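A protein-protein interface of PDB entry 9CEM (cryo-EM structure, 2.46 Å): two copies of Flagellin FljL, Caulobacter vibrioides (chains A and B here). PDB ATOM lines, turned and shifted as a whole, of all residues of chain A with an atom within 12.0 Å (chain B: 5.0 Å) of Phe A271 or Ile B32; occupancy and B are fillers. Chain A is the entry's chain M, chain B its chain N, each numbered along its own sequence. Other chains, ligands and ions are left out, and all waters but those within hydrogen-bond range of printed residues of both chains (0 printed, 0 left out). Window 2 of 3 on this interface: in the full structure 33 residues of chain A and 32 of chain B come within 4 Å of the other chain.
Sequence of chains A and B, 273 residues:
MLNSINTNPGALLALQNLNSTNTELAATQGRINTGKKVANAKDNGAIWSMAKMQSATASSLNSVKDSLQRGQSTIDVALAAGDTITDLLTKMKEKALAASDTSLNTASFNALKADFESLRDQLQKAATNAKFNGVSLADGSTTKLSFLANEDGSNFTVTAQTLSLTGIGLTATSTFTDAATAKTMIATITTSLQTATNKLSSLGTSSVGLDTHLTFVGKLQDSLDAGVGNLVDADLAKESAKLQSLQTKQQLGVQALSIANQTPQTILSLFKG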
ATOM      1  N   ASN A   3       7.814   7.321   6.267  1.00  0.00           N
ATOM      2  CA  ASN A   3       8.033   7.949   7.561  1.00  0.00           C
ATOM      3  C   ASN A   3       8.283   6.891   8.632  1.00  0.00           C
ATOM      4  O   ASN A   3       7.813   5.754   8.535  1.00  0.00           O
ATOM      5  CB  ASN A   3       6.856   8.863   7.933  1.00  0.00           C
ATOM      6  CG  ASN A   3       5.535   8.117   8.106  1.00  0.00           C
ATOM      7  OD1 ASN A   3       5.477   6.892   8.072  1.00  0.00           O
ATOM      8  ND2 ASN A   3       4.462   8.875   8.304  1.00  0.00           N
ATOM      9  N   SER A   4       9.073   7.263   9.640  1.00  0.00           N
ATOM     10  CA  SER A   4       9.435   6.335  10.701  1.00  0.00           C
ATOM     11  C   SER A   4       9.978   7.104  11.897  1.00  0.00           C
ATOM     12  O   SER A   4      10.634   8.137  11.735  1.00  0.00           O
ATOM     13  CB  SER A   4      10.468   5.317  10.212  1.00  0.00           C
ATOM     14  OG  SER A   4      11.693   5.959   9.907  1.00  0.00           O
ATOM     15  N   ILE A   5       9.708   6.580  13.099  1.00  0.00           N
ATOM     16  CA  ILE A   5      10.161   7.201  14.339  1.00  0.00           C
ATOM     17  C   ILE A   5      11.587   6.825  14.726  1.00  0.00           C
ATOM     18  O   ILE A   5      12.146   7.440  15.644  1.00  0.00           O
ATOM     19  CB  ILE A   5       9.175   6.852  15.474  1.00  0.00           C
ATOM     20  CG1 ILE A   5       9.134   5.338  15.692  1.00  0.00           C
ATOM     21  CG2 ILE A   5       7.801   7.425  15.194  1.00  0.00           C
ATOM     22  CD1 ILE A   5       8.374   4.914  16.919  1.00  0.00           C
ATOM     23  N   ASN A   6      12.199   5.845  14.062  1.00  0.00           N
ATOM     24  CA  ASN A   6      13.514   5.369  14.476  1.00  0.00           C
ATOM     25  C   ASN A   6      14.681   6.070  13.790  1.00  0.00           C
ATOM     26  O   ASN A   6      15.778   6.099  14.356  1.00  0.00           O
ATOM     27  CB  ASN A   6      13.629   3.859  14.244  1.00  0.00           C
ATOM     28  CG  ASN A   6      12.753   3.055  15.186  1.00  0.00           C
ATOM     29  OD1 ASN A   6      12.685   3.337  16.381  1.00  0.00           O
ATOM     30  ND2 ASN A   6      12.061   2.061  14.646  1.00  0.00           N
ATOM     31  N   THR A   7      14.490   6.632  12.596  1.00  0.00           N
ATOM     32  CA  THR A   7      15.589   7.282  11.892  1.00  0.00           C
ATOM     33  C   THR A   7      15.047   8.274  10.874  1.00  0.00           C
ATOM     34  O   THR A   7      13.900   8.170  10.430  1.00  0.00           O
ATOM     35  CB  THR A   7      16.497   6.263  11.183  1.00  0.00           C
ATOM     36  OG1 THR A   7      17.647   6.936  10.653  1.00  0.00           O
ATOM     37  CG2 THR A   7      15.758   5.577  10.046  1.00  0.00           C
ATOM     38  N   PRO A 264      10.079  14.606  12.018  1.00  0.00           N
ATOM     39  CA  PRO A 264       9.443  13.343  12.449  1.00  0.00           C
ATOM     40  C   PRO A 264       8.138  13.514  13.222  1.00  0.00           C
ATOM     41  O   PRO A 264       7.301  12.600  13.180  1.00  0.00           O
ATOM     42  CB  PRO A 264      10.505  12.697  13.343  1.00  0.00           C
ATOM     43  CG  PRO A 264      11.774  13.263  12.904  1.00  0.00           C
ATOM     44  CD  PRO A 264      11.461  14.681  12.528  1.00  0.00           C
ATOM     45  N   GLN A 265       7.952  14.625  13.937  1.00  0.00           N
ATOM     46  CA  GLN A 265       6.956  14.751  14.999  1.00  0.00           C
ATOM     47  C   GLN A 265       5.514  14.579  14.530  1.00  0.00           C
ATOM     48  O   GLN A 265       4.645  14.307  15.365  1.00  0.00           O
ATOM     49  CB  GLN A 265       7.110  16.111  15.687  1.00  0.00           C
ATOM     50  CG  GLN A 265       6.400  17.258  14.984  1.00  0.00           C
ATOM     51  CD  GLN A 265       6.911  18.618  15.425  1.00  0.00           C
ATOM     52  OE1 GLN A 265       7.400  18.778  16.545  1.00  0.00           O
ATOM     53  NE2 GLN A 265       6.795  19.607  14.547  1.00  0.00           N
ATOM     54  N   THR A 266       5.233  14.720  13.235  1.00  0.00           N
ATOM     55  CA  THR A 266       3.864  14.640  12.735  1.00  0.00           C
ATOM     56  C   THR A 266       3.231  13.265  12.911  1.00  0.00           C
ATOM     57  O   THR A 266       2.006  13.153  12.806  1.00  0.00           O
ATOM     58  CB  THR A 266       3.823  15.037  11.261  1.00  0.00           C
ATOM     59  OG1 THR A 266       4.215  13.918  10.455  1.00  0.00           O
ATOM     60  CG2 THR A 266       4.759  16.207  11.008  1.00  0.00           C
ATOM     61  N   ILE A 267       4.028  12.221  13.150  1.00  0.00           N
ATOM     62  CA  ILE A 267       3.477  10.881  13.345  1.00  0.00           C
ATOM     63  C   ILE A 267       2.575  10.839  14.573  1.00  0.00           C
ATOM     64  O   ILE A 267       1.660  10.008  14.654  1.00  0.00           O
ATOM     65  CB  ILE A 267       4.623   9.856  13.432  1.00  0.00           C
ATOM     66  CG1 ILE A 267       5.396   9.829  12.114  1.00  0.00           C
ATOM     67  CG2 ILE A 267       4.097   8.462  13.752  1.00  0.00           C
ATOM     68  CD1 ILE A 267       6.685   9.053  12.178  1.00  0.00           C
ATOM     69  N   LEU A 268       2.790  11.745  15.531  1.00  0.00           N
ATOM     70  CA  LEU A 268       1.927  11.811  16.706  1.00  0.00           C
ATOM     71  C   LEU A 268       0.480  12.100  16.330  1.00  0.00           C
ATOM     72  O   LEU A 268      -0.442  11.645  17.018  1.00  0.00           O
ATOM     73  CB  LEU A 268       2.432  12.892  17.658  1.00  0.00           C
ATOM     74  CG  LEU A 268       3.600  12.543  18.576  1.00  0.00           C
ATOM     75  CD1 LEU A 268       4.026  13.761  19.377  1.00  0.00           C
ATOM     76  CD2 LEU A 268       3.229  11.394  19.498  1.00  0.00           C
ATOM     77  N   SER A 269       0.259  12.849  15.248  1.00  0.00           N
ATOM     78  CA  SER A 269      -1.101  13.173  14.832  1.00  0.00           C
ATOM     79  C   SER A 269      -1.854  11.947  14.336  1.00  0.00           C
ATOM     80  O   SER A 269      -3.088  11.907  14.402  1.00  0.00           O
ATOM     81  CB  SER A 269      -1.071  14.249  13.748  1.00  0.00           C
ATOM     82  OG  SER A 269      -0.259  15.337  14.143  1.00  0.00           O
ATOM     83  N   LEU A 270      -1.136  10.944  13.826  1.00  0.00           N
ATOM     84  CA  LEU A 270      -1.783   9.771  13.252  1.00  0.00           C
ATOM     85  C   LEU A 270      -2.481   8.908  14.295  1.00  0.00           C
ATOM     86  O   LEU A 270      -3.362   8.120  13.937  1.00  0.00           O
ATOM     87  CB  LEU A 270      -0.764   8.929  12.485  1.00  0.00           C
ATOM     88  CG  LEU A 270      -0.195   9.558  11.213  1.00  0.00           C
ATOM     89  CD1 LEU A 270       1.234   9.098  10.995  1.00  0.00           C
ATOM     90  CD2 LEU A 270      -1.065   9.216  10.012  1.00  0.00           C
ATOM     91  N   PHE A 271      -2.107   9.024  15.564  1.00  0.00           N
ATOM     92  CA  PHE A 271      -2.671   8.160  16.592  1.00  0.00           C
ATOM     93  C   PHE A 271      -3.489   8.959  17.599  1.00  0.00           C
ATOM     94  O   PHE A 271      -3.410  10.186  17.643  1.00  0.00           O
ATOM     95  CB  PHE A 271      -1.560   7.388  17.306  1.00  0.00           C
ATOM     96  CG  PHE A 271      -0.787   6.469  16.406  1.00  0.00           C
ATOM     97  CD1 PHE A 271      -1.038   5.108  16.402  1.00  0.00           C
ATOM     98  CD2 PHE A 271       0.197   6.965  15.568  1.00  0.00           C
ATOM     99  CE1 PHE A 271      -0.330   4.262  15.574  1.00  0.00           C
ATOM    100  CE2 PHE A 271       0.909   6.124  14.739  1.00  0.00           C
ATOM    101  CZ  PHE A 271       0.646   4.770  14.742  1.00  0.00           C
ATOM    102  N   THR B  28       0.016  -5.951  15.328  1.00  0.00           N
ATOM    103  CA  THR B  28      -0.001  -4.566  14.879  1.00  0.00           C
ATOM    104  C   THR B  28       0.460  -3.627  15.984  1.00  0.00           C
ATOM    105  O   THR B  28       1.324  -2.771  15.757  1.00  0.00           O
ATOM    106  CB  THR B  28      -1.403  -4.187  14.401  1.00  0.00           C
ATOM    107  OG1 THR B  28      -1.705  -4.898  13.195  1.00  0.00           O
ATOM    108  CG2 THR B  28      -1.490  -2.694  14.128  1.00  0.00           C
ATOM    109  N   GLN B  29      -0.089  -3.778  17.193  1.00  0.00           N
ATOM    110  CA  GLN B  29       0.353  -2.928  18.290  1.00  0.00           C
ATOM    111  C   GLN B  29       1.805  -3.184  18.668  1.00  0.00           C
ATOM    112  O   GLN B  29       2.483  -2.257  19.130  1.00  0.00           O
ATOM    113  CB  GLN B  29      -0.541  -3.097  19.524  1.00  0.00           C
ATOM    114  CG  GLN B  29      -0.239  -4.300  20.396  1.00  0.00           C
ATOM    115  CD  GLN B  29      -1.436  -4.732  21.216  1.00  0.00           C
ATOM    116  OE1 GLN B  29      -2.565  -4.320  20.952  1.00  0.00           O
ATOM    117  NE2 GLN B  29      -1.192  -5.551  22.233  1.00  0.00           N
ATOM    118  N   GLY B  30       2.308  -4.404  18.466  1.00  0.00           N
ATOM    119  CA  GLY B  30       3.722  -4.638  18.697  1.00  0.00           C
ATOM    120  C   GLY B  30       4.597  -3.928  17.684  1.00  0.00           C
ATOM    121  O   GLY B  30       5.654  -3.392  18.029  1.00  0.00           O
ATOM    122  N   ARG B  31       4.161  -3.887  16.422  1.00  0.00           N
ATOM    123  CA  ARG B  31       4.906  -3.091  15.452  1.00  0.00           C
ATOM    124  C   ARG B  31       4.809  -1.601  15.753  1.00  0.00           C
ATOM    125  O   ARG B  31       5.742  -0.851  15.453  1.00  0.00           O
ATOM    126  CB  ARG B  31       4.433  -3.363  14.027  1.00  0.00           C
ATOM    127  CG  ARG B  31       4.774  -4.741  13.508  1.00  0.00           C
ATOM    128  CD  ARG B  31       4.566  -4.806  12.006  1.00  0.00           C
ATOM    129  NE  ARG B  31       3.160  -4.756  11.623  1.00  0.00           N
ATOM    130  CZ  ARG B  31       2.278  -5.721  11.841  1.00  0.00           C
ATOM    131  NH1 ARG B  31       2.615  -6.845  12.449  1.00  0.00           N
ATOM    132  NH2 ARG B  31       1.023  -5.554  11.433  1.00  0.00           N
ATOM    133  N   ILE B  32       3.693  -1.152  16.331  1.00  0.00           N
ATOM    134  CA  ILE B  32       3.573   0.263  16.677  1.00  0.00           C
ATOM    135  C   ILE B  32       4.526   0.622  17.810  1.00  0.00           C
ATOM    136  O   ILE B  32       5.296   1.584  17.708  1.00  0.00           O
ATOM    137  CB  ILE B  32       2.119   0.627  17.029  1.00  0.00           C
ATOM    138  CG1 ILE B  32       1.169   0.229  15.900  1.00  0.00           C
ATOM    139  CG2 ILE B  32       2.007   2.112  17.358  1.00  0.00           C
ATOM    140  CD1 ILE B  32      -0.287   0.520  16.193  1.00  0.00           C
ATOM    141  N   ASN B  33       4.492  -0.139  18.908  1.00  0.00           N
ATOM    142  CA  ASN B  33       5.362   0.205  20.028  1.00  0.00           C
ATOM    143  C   ASN B  33       6.836   0.005  19.693  1.00  0.00           C
ATOM    144  O   ASN B  33       7.673   0.807  20.120  1.00  0.00           O
ATOM    145  CB  ASN B  33       4.991  -0.601  21.279  1.00  0.00           C
ATOM    146  CG  ASN B  33       5.038  -2.100  21.057  1.00  0.00           C
ATOM    147  OD1 ASN B  33       6.017  -2.635  20.544  1.00  0.00           O
ATOM    148  ND2 ASN B  33       3.977  -2.787  21.460  1.00  0.00           N
ATOM    149  N   THR B  34       7.174  -1.043  18.933  1.00  0.00           N
ATOM    150  CA  THR B  34       8.571  -1.264  18.569  1.00  0.00           C
ATOM    151  C   THR B  34       9.071  -0.210  17.590  1.00  0.00           C
ATOM    152  O   THR B  34      10.258   0.134  17.591  1.00  0.00           O
ATOM    153  CB  THR B  34       8.748  -2.658  17.969  1.00  0.00           C
ATOM    154  OG1 THR B  34       7.666  -2.931  17.073  1.00  0.00           O
ATOM    155  CG2 THR B  34       8.768  -3.714  19.061  1.00  0.00           C
ATOM    156  N   GLY B  35       8.184   0.308  16.744  1.00  0.00           N
ATOM    157  CA  GLY B  35       8.602   1.170  15.658  1.00  0.00           C
ATOM    158  C   GLY B  35       9.239   0.441  14.498  1.00  0.00           C
ATOM    159  O   GLY B  35       9.797   1.092  13.608  1.00  0.00           O
ATOM    160  N   LEU B 236       4.619   3.769   9.884  1.00  0.00           N
ATOM    161  CA  LEU B 236       3.575   3.844  10.902  1.00  0.00           C
ATOM    162  C   LEU B 236       2.256   4.422  10.400  1.00  0.00           C
ATOM    163  O   LEU B 236       1.210   4.143  11.002  1.00  0.00           O
ATOM    164  CB  LEU B 236       4.085   4.668  12.081  1.00  0.00           C
ATOM    165  CG  LEU B 236       5.128   3.928  12.917  1.00  0.00           C
ATOM    166  CD1 LEU B 236       5.644   4.820  14.013  1.00  0.00           C
ATOM    167  CD2 LEU B 236       4.532   2.659  13.501  1.00  0.00           C
ATOM    168  N   GLU B 239       0.370   1.519   9.712  1.00  0.00           N
ATOM    169  CA  GLU B 239       0.054   0.804  10.942  1.00  0.00           C
ATOM    170  C   GLU B 239      -1.140   1.414  11.663  1.00  0.00           C
ATOM    171  O   GLU B 239      -1.934   0.681  12.259  1.00  0.00           O
ATOM    172  CB  GLU B 239       1.270   0.781  11.874  1.00  0.00           C
ATOM    173  CG  GLU B 239       2.597   0.329  11.255  1.00  0.00           C
ATOM    174  CD  GLU B 239       2.511  -0.976  10.476  1.00  0.00           C
ATOM    175  OE1 GLU B 239       3.356  -1.183   9.582  1.00  0.00           O
ATOM    176  OE2 GLU B 239       1.637  -1.816  10.783  1.00  0.00           O
ATOM    177  N   SER B 240      -1.299   2.739  11.612  1.00  0.00           N
ATOM    178  CA  SER B 240      -2.457   3.351  12.259  1.00  0.00           C
ATOM    179  C   SER B 240      -3.756   2.957  11.560  1.00  0.00           C
ATOM    180  O   SER B 240      -4.770   2.682  12.219  1.00  0.00           O
ATOM    181  CB  SER B 240      -2.297   4.869  12.289  1.00  0.00           C
ATOM    182  OG  SER B 240      -2.230   5.402  10.977  1.00  0.00           O
ATOM    183  N   LEU B 243      -4.536  -0.464  12.519  1.00  0.00           N
ATOM    184  CA  LEU B 243      -5.013  -0.490  13.896  1.00  0.00           C
ATOM    185  C   LEU B 243      -6.502  -0.177  13.967  1.00  0.00           C
ATOM    186  O   LEU B 243      -7.276  -0.915  14.591  1.00  0.00           O
ATOM    187  CB  LEU B 243      -4.212   0.512  14.730  1.00  0.00           C
ATOM    188  CG  LEU B 243      -4.600   0.747  16.192  1.00  0.00           C
ATOM    189  CD1 LEU B 243      -4.524  -0.532  17.001  1.00  0.00           C
ATOM    190  CD2 LEU B 243      -3.724   1.826  16.803  1.00  0.00           C
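ND2 of Asn A6 is in hydrogen-bond range of O of Gly B35 (2.7 Å).
The side-chain hydroxyl (OG1) of Thr B34 sits close to the backbone carbonyl oxygen (O) of Arg B31 (3.3 Å).
Among the printed residues, pairs that only touch across the chains: Ile A5 with Leu B236, Phe A271 with Ile B32, Asn A3 with Leu B236, Leu A270 with Ser B240, Phe A271 with Ser B240, Phe A271 with Leu B236, Asn A6 with Thr B34, Ile A5 with Gly B35 and Ile A267 with Leu B236.
Of chain B, only Ile B32, Leu B236 and Ser B240 come within 4 Å of Phe A271. Ile B32 touches just one residue of chain A: Phe A271. No residue of chain A comes within 4 Å of Thr B28. No residue of chain A comes within 4 Å of Gly B30. Arg B31 touches none of the printed residues of chain A. No residue of chain A comes within 4 Å of Asn B33. Of chain A, only Asn A6 comes within 4 Å of Thr B34. Gly B35 touches just these residues of chain A: Ile A5 and Asn A6. Leu B236 touches four residues of chain A. No residue of chain A comes within 4 Å of Glu B239. Ser B240 touches just these residues of chain A: Leu A270 and Phe A271. No residue of chain A comes within 4 Å of Leu B243. Printed residues of chain B within 4 Å of Ile A267: Leu B236. Of the printed residues of chain B, Ile A5 touches Gly B35 (3.96 Å) and Leu B236 (3.6 Å). Printed residues of chain B within 4 Å of Asn A6: Thr B34 and Gly B35. Of the printed residues of chain B, Leu A270 touches Ser B240 (3.8 Å). Of the printed residues of chain B, Asn A3 touches Leu B236. The nearest residue of chain A that does not touch Ile B32 is Ile A5 (4.6 Å).
Of the 12 printed residues of chain B, 5 touch a printed residue of chain A. Printed residues of chain A that touch a printed residue of chain B: Asn A3, Ile A5, Asn A6, Ile A267, Leu A270 and Phe A271. Among the printed residues, 10 pairs touch across the chains.
No position is printed for both chains.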
